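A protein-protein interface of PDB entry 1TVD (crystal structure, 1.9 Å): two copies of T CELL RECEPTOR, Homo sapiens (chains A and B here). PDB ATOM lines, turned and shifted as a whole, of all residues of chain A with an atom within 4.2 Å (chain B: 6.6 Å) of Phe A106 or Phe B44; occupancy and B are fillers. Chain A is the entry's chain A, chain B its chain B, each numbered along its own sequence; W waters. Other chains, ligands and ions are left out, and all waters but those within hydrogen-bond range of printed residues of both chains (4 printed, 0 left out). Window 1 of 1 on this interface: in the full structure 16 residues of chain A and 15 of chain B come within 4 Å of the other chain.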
ATOM      1  N   VAL A   3      28.908   3.378  -4.768  1.00  0.00           N
ATOM      2  CA  VAL A   3      27.478   3.652  -4.800  1.00  0.00           C
ATOM      3  C   VAL A   3      27.076   3.815  -3.345  1.00  0.00           C
ATOM      4  O   VAL A   3      27.395   2.964  -2.503  1.00  0.00           O
ATOM      5  CB  VAL A   3      26.654   2.473  -5.389  1.00  0.00           C
ATOM      6  CG1 VAL A   3      25.165   2.808  -5.395  1.00  0.00           C
ATOM      7  CG2 VAL A   3      27.130   2.134  -6.783  1.00  0.00           C
ATOM      8  N   TYR A  36      17.695  -2.689  -8.603  1.00  0.00           N
ATOM      9  CA  TYR A  36      17.292  -4.094  -8.589  1.00  0.00           C
ATOM     10  C   TYR A  36      16.748  -4.363  -7.204  1.00  0.00           C
ATOM     11  O   TYR A  36      17.049  -3.620  -6.269  1.00  0.00           O
ATOM     12  CB  TYR A  36      18.508  -4.998  -8.816  1.00  0.00           C
ATOM     13  CG  TYR A  36      18.915  -5.157 -10.268  1.00  0.00           C
ATOM     14  CD1 TYR A  36      18.238  -6.046 -11.111  1.00  0.00           C
ATOM     15  CD2 TYR A  36      19.979  -4.431 -10.797  1.00  0.00           C
ATOM     16  CE1 TYR A  36      18.619  -6.202 -12.441  1.00  0.00           C
ATOM     17  CE2 TYR A  36      20.360  -4.584 -12.116  1.00  0.00           C
ATOM     18  CZ  TYR A  36      19.680  -5.467 -12.927  1.00  0.00           C
ATOM     19  OH  TYR A  36      20.092  -5.611 -14.215  1.00  0.00           O
ATOM     20  N   PHE A  44      15.873 -12.134  -7.808  1.00  0.00           N
ATOM     21  CA  PHE A  44      16.189 -10.741  -8.053  1.00  0.00           C
ATOM     22  C   PHE A  44      15.272 -10.258  -9.171  1.00  0.00           C
ATOM     23  O   PHE A  44      14.861 -11.042 -10.033  1.00  0.00           O
ATOM     24  CB  PHE A  44      17.657 -10.597  -8.474  1.00  0.00           C
ATOM     25  CG  PHE A  44      18.527  -9.881  -7.458  1.00  0.00           C
ATOM     26  CD1 PHE A  44      18.344  -8.522  -7.196  1.00  0.00           C
ATOM     27  CD2 PHE A  44      19.561 -10.549  -6.809  1.00  0.00           C
ATOM     28  CE1 PHE A  44      19.180  -7.839  -6.310  1.00  0.00           C
ATOM     29  CE2 PHE A  44      20.406  -9.877  -5.916  1.00  0.00           C
ATOM     30  CZ  PHE A  44      20.213  -8.513  -5.669  1.00  0.00           C
ATOM     31  N   CYS A  93      21.139  -0.409  -5.711  1.00  0.00           N
ATOM     32  CA  CYS A  93      21.441   0.547  -6.749  1.00  0.00           C
ATOM     33  C   CYS A  93      22.834   0.167  -7.262  1.00  0.00           C
ATOM     34  O   CYS A  93      23.680  -0.343  -6.494  1.00  0.00           O
ATOM     35  CB  CYS A  93      21.446   1.949  -6.166  1.00  0.00           C
ATOM     36  SG  CYS A  93      21.629   3.263  -7.394  1.00  0.00           S
ATOM     37  N   ALA A  94      23.064   0.360  -8.558  1.00  0.00           N
ATOM     38  CA  ALA A  94      24.349   0.003  -9.170  1.00  0.00           C
ATOM     39  C   ALA A  94      24.543   0.738 -10.478  1.00  0.00           C
ATOM     40  O   ALA A  94      23.576   1.198 -11.091  1.00  0.00           O
ATOM     41  CB  ALA A  94      24.402  -1.525  -9.433  1.00  0.00           C
ATOM     42  N   LEU A 104      28.933  -4.439 -13.160  1.00  0.00           N
ATOM     43  CA  LEU A 104      28.264  -3.603 -12.166  1.00  0.00           C
ATOM     44  C   LEU A 104      28.976  -3.428 -10.849  1.00  0.00           C
ATOM     45  O   LEU A 104      29.701  -4.318 -10.397  1.00  0.00           O
ATOM     46  CB  LEU A 104      26.874  -4.177 -11.868  1.00  0.00           C
ATOM     47  CG  LEU A 104      25.856  -4.243 -13.008  1.00  0.00           C
ATOM     48  CD1 LEU A 104      24.680  -5.105 -12.608  1.00  0.00           C
ATOM     49  CD2 LEU A 104      25.404  -2.853 -13.376  1.00  0.00           C
ATOM     50  N   ILE A 105      28.764  -2.259 -10.252  1.00  0.00           N
ATOM     51  CA  ILE A 105      29.299  -1.919  -8.933  1.00  0.00           C
ATOM     52  C   ILE A 105      28.023  -1.698  -8.140  1.00  0.00           C
ATOM     53  O   ILE A 105      27.177  -0.899  -8.556  1.00  0.00           O
ATOM     54  CB  ILE A 105      30.136  -0.621  -8.971  1.00  0.00           C
ATOM     55  CG1 ILE A 105      31.403  -0.854  -9.818  1.00  0.00           C
ATOM     56  CG2 ILE A 105      30.497  -0.174  -7.537  1.00  0.00           C
ATOM     57  CD1 ILE A 105      32.388   0.311  -9.826  1.00  0.00           C
ATOM     58  N   PHE A 106      27.847  -2.434  -7.044  1.00  0.00           N
ATOM     59  CA  PHE A 106      26.615  -2.317  -6.252  1.00  0.00           C
ATOM     60  C   PHE A 106      26.681  -1.499  -4.969  1.00  0.00           C
ATOM     61  O   PHE A 106      27.738  -1.352  -4.345  1.00  0.00           O
ATOM     62  CB  PHE A 106      26.083  -3.701  -5.867  1.00  0.00           C
ATOM     63  CG  PHE A 106      25.715  -4.570  -7.030  1.00  0.00           C
ATOM     64  CD1 PHE A 106      26.684  -5.325  -7.689  1.00  0.00           C
ATOM     65  CD2 PHE A 106      24.388  -4.677  -7.443  1.00  0.00           C
ATOM     66  CE1 PHE A 106      26.345  -6.169  -8.728  1.00  0.00           C
ATOM     67  CE2 PHE A 106      24.036  -5.529  -8.492  1.00  0.00           C
ATOM     68  CZ  PHE A 106      25.021  -6.275  -9.133  1.00  0.00           C
ATOM     69  N   GLY A 107      25.524  -0.965  -4.593  1.00  0.00           N
ATOM     70  CA  GLY A 107      25.402  -0.240  -3.348  1.00  0.00           C
ATOM     71  C   GLY A 107      25.204  -1.322  -2.285  1.00  0.00           C
ATOM     72  O   GLY A 107      25.021  -2.501  -2.636  1.00  0.00           O
ATOM     73  N   TYR B  36      24.691 -15.584  -9.273  1.00  0.00           N
ATOM     74  CA  TYR B  36      23.625 -14.903  -9.996  1.00  0.00           C
ATOM     75  C   TYR B  36      24.222 -14.503 -11.331  1.00  0.00           C
ATOM     76  O   TYR B  36      25.449 -14.403 -11.458  1.00  0.00           O
ATOM     77  CB  TYR B  36      23.186 -13.628  -9.263  1.00  0.00           C
ATOM     78  CG  TYR B  36      22.287 -13.854  -8.069  1.00  0.00           C
ATOM     79  CD1 TYR B  36      20.895 -13.904  -8.217  1.00  0.00           C
ATOM     80  CD2 TYR B  36      22.816 -13.972  -6.783  1.00  0.00           C
ATOM     81  CE1 TYR B  36      20.055 -14.063  -7.113  1.00  0.00           C
ATOM     82  CE2 TYR B  36      21.988 -14.132  -5.681  1.00  0.00           C
ATOM     83  CZ  TYR B  36      20.609 -14.178  -5.853  1.00  0.00           C
ATOM     84  OH  TYR B  36      19.785 -14.361  -4.769  1.00  0.00           O
ATOM     85  N   ARG B  37      23.374 -14.278 -12.328  1.00  0.00           N
ATOM     86  CA  ARG B  37      23.874 -13.864 -13.633  1.00  0.00           C
ATOM     87  C   ARG B  37      23.019 -12.780 -14.251  1.00  0.00           C
ATOM     88  O   ARG B  37      21.787 -12.781 -14.109  1.00  0.00           O
ATOM     89  CB  ARG B  37      23.985 -15.053 -14.585  1.00  0.00           C
ATOM     90  CG  ARG B  37      22.665 -15.687 -14.971  1.00  0.00           C
ATOM     91  CD  ARG B  37      22.887 -16.885 -15.862  1.00  0.00           C
ATOM     92  NE  ARG B  37      21.628 -17.436 -16.366  1.00  0.00           N
ATOM     93  CZ  ARG B  37      21.554 -18.461 -17.202  1.00  0.00           C
ATOM     94  NH1 ARG B  37      22.667 -19.047 -17.628  1.00  0.00           N
ATOM     95  NH2 ARG B  37      20.377 -18.915 -17.589  1.00  0.00           N
ATOM     96  N   ILE B  38      23.684 -11.809 -14.867  1.00  0.00           N
ATOM     97  CA  ILE B  38      23.004 -10.715 -15.533  1.00  0.00           C
ATOM     98  C   ILE B  38      22.954 -11.054 -17.017  1.00  0.00           C
ATOM     99  O   ILE B  38      24.006 -11.211 -17.659  1.00  0.00           O
ATOM    100  CB  ILE B  38      23.764  -9.372 -15.372  1.00  0.00           C
ATOM    101  CG1 ILE B  38      23.762  -8.915 -13.911  1.00  0.00           C
ATOM    102  CG2 ILE B  38      23.094  -8.289 -16.221  1.00  0.00           C
ATOM    103  CD1 ILE B  38      22.539  -8.107 -13.526  1.00  0.00           C
ATOM    104  N   ARG B  39      21.738 -11.205 -17.538  1.00  0.00           N
ATOM    105  CA  ARG B  39      21.504 -11.511 -18.947  1.00  0.00           C
ATOM    106  C   ARG B  39      21.480 -10.199 -19.732  1.00  0.00           C
ATOM    107  O   ARG B  39      21.211  -9.140 -19.166  1.00  0.00           O
ATOM    108  CB  ARG B  39      20.177 -12.253 -19.116  1.00  0.00           C
ATOM    109  CG  ARG B  39      20.119 -13.581 -18.381  1.00  0.00           C
ATOM    110  CD  ARG B  39      19.241 -14.570 -19.129  1.00  0.00           C
ATOM    111  NE  ARG B  39      19.657 -14.707 -20.528  1.00  0.00           N
ATOM    112  CZ  ARG B  39      20.843 -15.175 -20.929  1.00  0.00           C
ATOM    113  NH1 ARG B  39      21.750 -15.568 -20.042  1.00  0.00           N
ATOM    114  NH2 ARG B  39      21.143 -15.200 -22.224  1.00  0.00           N
ATOM    115  N   ASP B  41      19.354  -8.702 -21.442  1.00  0.00           N
ATOM    116  CA  ASP B  41      18.140  -7.900 -21.265  1.00  0.00           C
ATOM    117  C   ASP B  41      17.983  -7.311 -19.847  1.00  0.00           C
ATOM    118  O   ASP B  41      16.902  -6.864 -19.482  1.00  0.00           O
ATOM    119  CB  ASP B  41      16.882  -8.700 -21.661  1.00  0.00           C
ATOM    120  CG  ASP B  41      16.579  -9.863 -20.702  1.00  0.00           C
ATOM    121  OD1 ASP B  41      17.394 -10.176 -19.802  1.00  0.00           O
ATOM    122  OD2 ASP B  41      15.509 -10.471 -20.856  1.00  0.00           O
ATOM    123  N   TYR B  42      19.056  -7.362 -19.052  1.00  0.00           N
ATOM    124  CA  TYR B  42      19.065  -6.821 -17.690  1.00  0.00           C
ATOM    125  C   TYR B  42      18.483  -7.716 -16.589  1.00  0.00           C
ATOM    126  O   TYR B  42      18.551  -7.366 -15.407  1.00  0.00           O
ATOM    127  CB  TYR B  42      18.371  -5.449 -17.628  1.00  0.00           C
ATOM    128  CG  TYR B  42      18.972  -4.388 -18.510  1.00  0.00           C
ATOM    129  CD1 TYR B  42      20.322  -4.407 -18.833  1.00  0.00           C
ATOM    130  CD2 TYR B  42      18.189  -3.345 -18.996  1.00  0.00           C
ATOM    131  CE1 TYR B  42      20.889  -3.406 -19.617  1.00  0.00           C
ATOM    132  CE2 TYR B  42      18.736  -2.336 -19.778  1.00  0.00           C
ATOM    133  CZ  TYR B  42      20.089  -2.367 -20.085  1.00  0.00           C
ATOM    134  OH  TYR B  42      20.639  -1.339 -20.843  1.00  0.00           O
ATOM    135  N   SER B  43      17.835  -8.813 -16.957  1.00  0.00           N
ATOM    136  CA  SER B  43      17.289  -9.697 -15.937  1.00  0.00           C
ATOM    137  C   SER B  43      18.438 -10.225 -15.094  1.00  0.00           C
ATOM    138  O   SER B  43      19.524 -10.483 -15.616  1.00  0.00           O
ATOM    139  CB  SER B  43      16.537 -10.862 -16.568  1.00  0.00           C
ATOM    140  OG  SER B  43      17.394 -11.681 -17.345  1.00  0.00           O
ATOM    141  N   PHE B  44      18.223 -10.284 -13.783  1.00  0.00           N
ATOM    142  CA  PHE B  44      19.221 -10.767 -12.832  1.00  0.00           C
ATOM    143  C   PHE B  44      18.672 -12.114 -12.356  1.00  0.00           C
ATOM    144  O   PHE B  44      17.720 -12.158 -11.583  1.00  0.00           O
ATOM    145  CB  PHE B  44      19.327  -9.768 -11.665  1.00  0.00           C
ATOM    146  CG  PHE B  44      20.660  -9.777 -10.957  1.00  0.00           C
ATOM    147  CD1 PHE B  44      21.659 -10.663 -11.333  1.00  0.00           C
ATOM    148  CD2 PHE B  44      20.917  -8.875  -9.927  1.00  0.00           C
ATOM    149  CE1 PHE B  44      22.893 -10.654 -10.700  1.00  0.00           C
ATOM    150  CE2 PHE B  44      22.147  -8.859  -9.286  1.00  0.00           C
ATOM    151  CZ  PHE B  44      23.139  -9.752  -9.673  1.00  0.00           C
ATOM    152  N   GLN B  45      19.274 -13.203 -12.834  1.00  0.00           N
ATOM    153  CA  GLN B  45      18.834 -14.562 -12.520  1.00  0.00           C
ATOM    154  C   GLN B  45      19.560 -15.307 -11.419  1.00  0.00           C
ATOM    155  O   GLN B  45      20.788 -15.377 -11.417  1.00  0.00           O
ATOM    156  CB  GLN B  45      18.949 -15.445 -13.764  1.00  0.00           C
ATOM    157  CG  GLN B  45      17.780 -15.469 -14.677  1.00  0.00           C
ATOM    158  CD  GLN B  45      17.840 -16.668 -15.606  1.00  0.00           C
ATOM    159  OE1 GLN B  45      18.744 -16.780 -16.438  1.00  0.00           O
ATOM    160  NE2 GLN B  45      16.916 -17.606 -15.423  1.00  0.00           N
ATOM    161  N   PHE B  46      18.787 -15.970 -10.563  1.00  0.00           N
ATOM    162  CA  PHE B  46      19.343 -16.792  -9.496  1.00  0.00           C
ATOM    163  C   PHE B  46      19.828 -18.090 -10.154  1.00  0.00           C
ATOM    164  O   PHE B  46      19.089 -18.710 -10.916  1.00  0.00           O
ATOM    165  CB  PHE B  46      18.265 -17.139  -8.450  1.00  0.00           C
ATOM    166  CG  PHE B  46      18.684 -18.224  -7.477  1.00  0.00           C
ATOM    167  CD1 PHE B  46      19.656 -17.978  -6.511  1.00  0.00           C
ATOM    168  CD2 PHE B  46      18.135 -19.499  -7.560  1.00  0.00           C
ATOM    169  CE1 PHE B  46      20.076 -18.987  -5.650  1.00  0.00           C
ATOM    170  CE2 PHE B  46      18.553 -20.511  -6.709  1.00  0.00           C
ATOM    171  CZ  PHE B  46      19.525 -20.255  -5.751  1.00  0.00           C
ATOM    172  N   THR B  90      26.837 -12.285 -17.502  1.00  0.00           N
ATOM    173  CA  THR B  90      27.930 -11.950 -16.599  1.00  0.00           C
ATOM    174  C   THR B  90      27.538 -12.564 -15.255  1.00  0.00           C
ATOM    175  O   THR B  90      26.464 -12.285 -14.706  1.00  0.00           O
ATOM    176  CB  THR B  90      28.129 -10.443 -16.466  1.00  0.00           C
ATOM    177  OG1 THR B  90      28.407  -9.898 -17.760  1.00  0.00           O
ATOM    178  CG2 THR B  90      29.295 -10.143 -15.534  1.00  0.00           C
ATOM    179  N   TYR B  92      27.966 -13.374 -11.307  1.00  0.00           N
ATOM    180  CA  TYR B  92      28.379 -12.757 -10.055  1.00  0.00           C
ATOM    181  C   TYR B  92      28.282 -13.734  -8.905  1.00  0.00           C
ATOM    182  O   TYR B  92      27.225 -14.323  -8.657  1.00  0.00           O
ATOM    183  CB  TYR B  92      27.491 -11.542  -9.726  1.00  0.00           C
ATOM    184  CG  TYR B  92      27.667 -10.385 -10.675  1.00  0.00           C
ATOM    185  CD1 TYR B  92      26.908 -10.293 -11.836  1.00  0.00           C
ATOM    186  CD2 TYR B  92      28.634  -9.407 -10.441  1.00  0.00           C
ATOM    187  CE1 TYR B  92      27.111  -9.260 -12.747  1.00  0.00           C
ATOM    188  CE2 TYR B  92      28.843  -8.365 -11.349  1.00  0.00           C
ATOM    189  CZ  TYR B  92      28.076  -8.308 -12.500  1.00  0.00           C
ATOM    190  OH  TYR B  92      28.281  -7.304 -13.422  1.00  0.00           O
ATOM    191  N   LEU B 104      23.746  -8.399   0.723  1.00  0.00           N
ATOM    192  CA  LEU B 104      24.723  -9.026  -0.158  1.00  0.00           C
ATOM    193  C   LEU B 104      26.026  -8.284  -0.419  1.00  0.00           C
ATOM    194  O   LEU B 104      26.048  -7.049  -0.552  1.00  0.00           O
ATOM    195  CB  LEU B 104      24.066  -9.308  -1.513  1.00  0.00           C
ATOM    196  CG  LEU B 104      22.951 -10.354  -1.589  1.00  0.00           C
ATOM    197  CD1 LEU B 104      22.037 -10.016  -2.734  1.00  0.00           C
ATOM    198  CD2 LEU B 104      23.559 -11.746  -1.745  1.00  0.00           C
ATOM    199  N   PHE B 106      28.923  -8.528  -3.239  1.00  0.00           N
ATOM    200  CA  PHE B 106      29.132  -9.078  -4.585  1.00  0.00           C
ATOM    201  C   PHE B 106      30.577  -9.082  -5.082  1.00  0.00           C
ATOM    202  O   PHE B 106      31.393  -8.244  -4.691  1.00  0.00           O
ATOM    203  CB  PHE B 106      28.314  -8.279  -5.624  1.00  0.00           C
ATOM    204  CG  PHE B 106      26.834  -8.548  -5.598  1.00  0.00           C
ATOM    205  CD1 PHE B 106      26.298  -9.610  -6.318  1.00  0.00           C
ATOM    206  CD2 PHE B 106      25.966  -7.679  -4.942  1.00  0.00           C
ATOM    207  CE1 PHE B 106      24.903  -9.799  -6.397  1.00  0.00           C
ATOM    208  CE2 PHE B 106      24.569  -7.856  -5.011  1.00  0.00           C
ATOM    209  CZ  PHE B 106      24.041  -8.919  -5.745  1.00  0.00           C
ATOM    210  N   GLY B 107      30.866 -10.025  -5.963  1.00  0.00           N
ATOM    211  CA  GLY B 107      32.174 -10.093  -6.575  1.00  0.00           C
ATOM    212  C   GLY B 107      32.063  -9.141  -7.762  1.00  0.00           C
ATOM    213  O   GLY B 107      30.976  -8.604  -8.027  1.00  0.00           O
HETATM  214  O   HOH W   1      30.368  -5.813  -8.076  1.00  0.00           O
HETATM  215  O   HOH W   2      26.640  -4.879  -2.041  1.00  0.00           O
HETATM  216  O   HOH W   3      16.468 -14.127  -9.889  1.00  0.00           O
HETATM  217  O   HOH W   4      15.389  -9.773 -12.841  1.00  0.00           O
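N of Tyr B92 sits at hydrogen-bond distance from O of Tyr B36 (2.7 Å).
The backbone carbonyl oxygen (O) of Thr B90 sits at hydrogen-bond distance from the backbone NH (N) of Ile B38.
Along chain A the printed residues that touch a printed residue of chain B span positions 36 to 106.
Of the 15 printed residues of chain B, 7 touch a printed residue of chain A.
Among the printed residues, no Asp or Glu carboxylate lies within 4 Å of a Lys or Arg side-chain nitrogen of the other chain.
Water W2 lies within hydrogen-bond range of O of Leu B104 (2.7 Å) and O of Gly A107 (2.9 Å).
Water W1 lies within hydrogen-bond range of O of Leu A104 (2.8 Å) and O of Gly B107 (2.9 Å).
Water W3 lies within hydrogen-bond range of O of Phe B44 (2.9 Å), N of Phe A44 (2.9 Å) and N of Phe B46 (3.0 Å).
Water W4 lies within hydrogen-bond range of N of Phe B44 and O of Phe A44.
The side-chain hydroxyl (OH) of Tyr B92 is in hydrogen-bond range of the backbone NH (N) of Leu A104 (2.9 Å).
O of Phe A44 sits close to O of Phe B44 (3.4 Å).
OH of Tyr A36 lies within hydrogen-bond range of O of Tyr B42 (2.6 Å).
Tyr A36 touches Phe B44, and with the chains exchanged Phe A44 touches Tyr B36.
Phe A44 touches Leu B104, but with the chains exchanged Leu A104 does not touch Phe B44 (5.6 Å).
Phe A44 touches Phe B106, and with the chains exchanged Phe A106 touches Phe B44.
Phe A106 touches its own counterpart, Phe B106.
Positions printed for both chains: 36, 44, 104, 106 and 107.
Phe A106 touches just these residues of chain B: Phe B44 and Phe B106.
Phe B44 touches three residues of chain A.
Of the printed residues of chain B, Leu A104 touches Ile B38 and Tyr B92.
Of the printed residues of chain A, Tyr B42 touches Tyr A36 (2.6 Å).
Cys A93 touches none of the printed residues of chain B.
The nearest printed residue of chain A that does not touch Tyr B36 is Phe A106 (7.6 Å).
Ile B38 touches Tyr A36.
Tyr A36 touches Phe B44 (CE1 to CB, 3.7 Å).
CD2 of Phe A44 touches CE1 of Tyr B36, at 3.6 Å.
Leu B104 touches Phe A44 (CD1 to CE2, 3.6 Å).
Phe A44 touches Phe B106.
CD1 of Ile B38 touches CD1 of Leu A104 (3.8 Å).
Phe A106 touches Phe B44.
CD2 of Phe B106 touches CD1 of Phe A106, at 3.7 Å.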
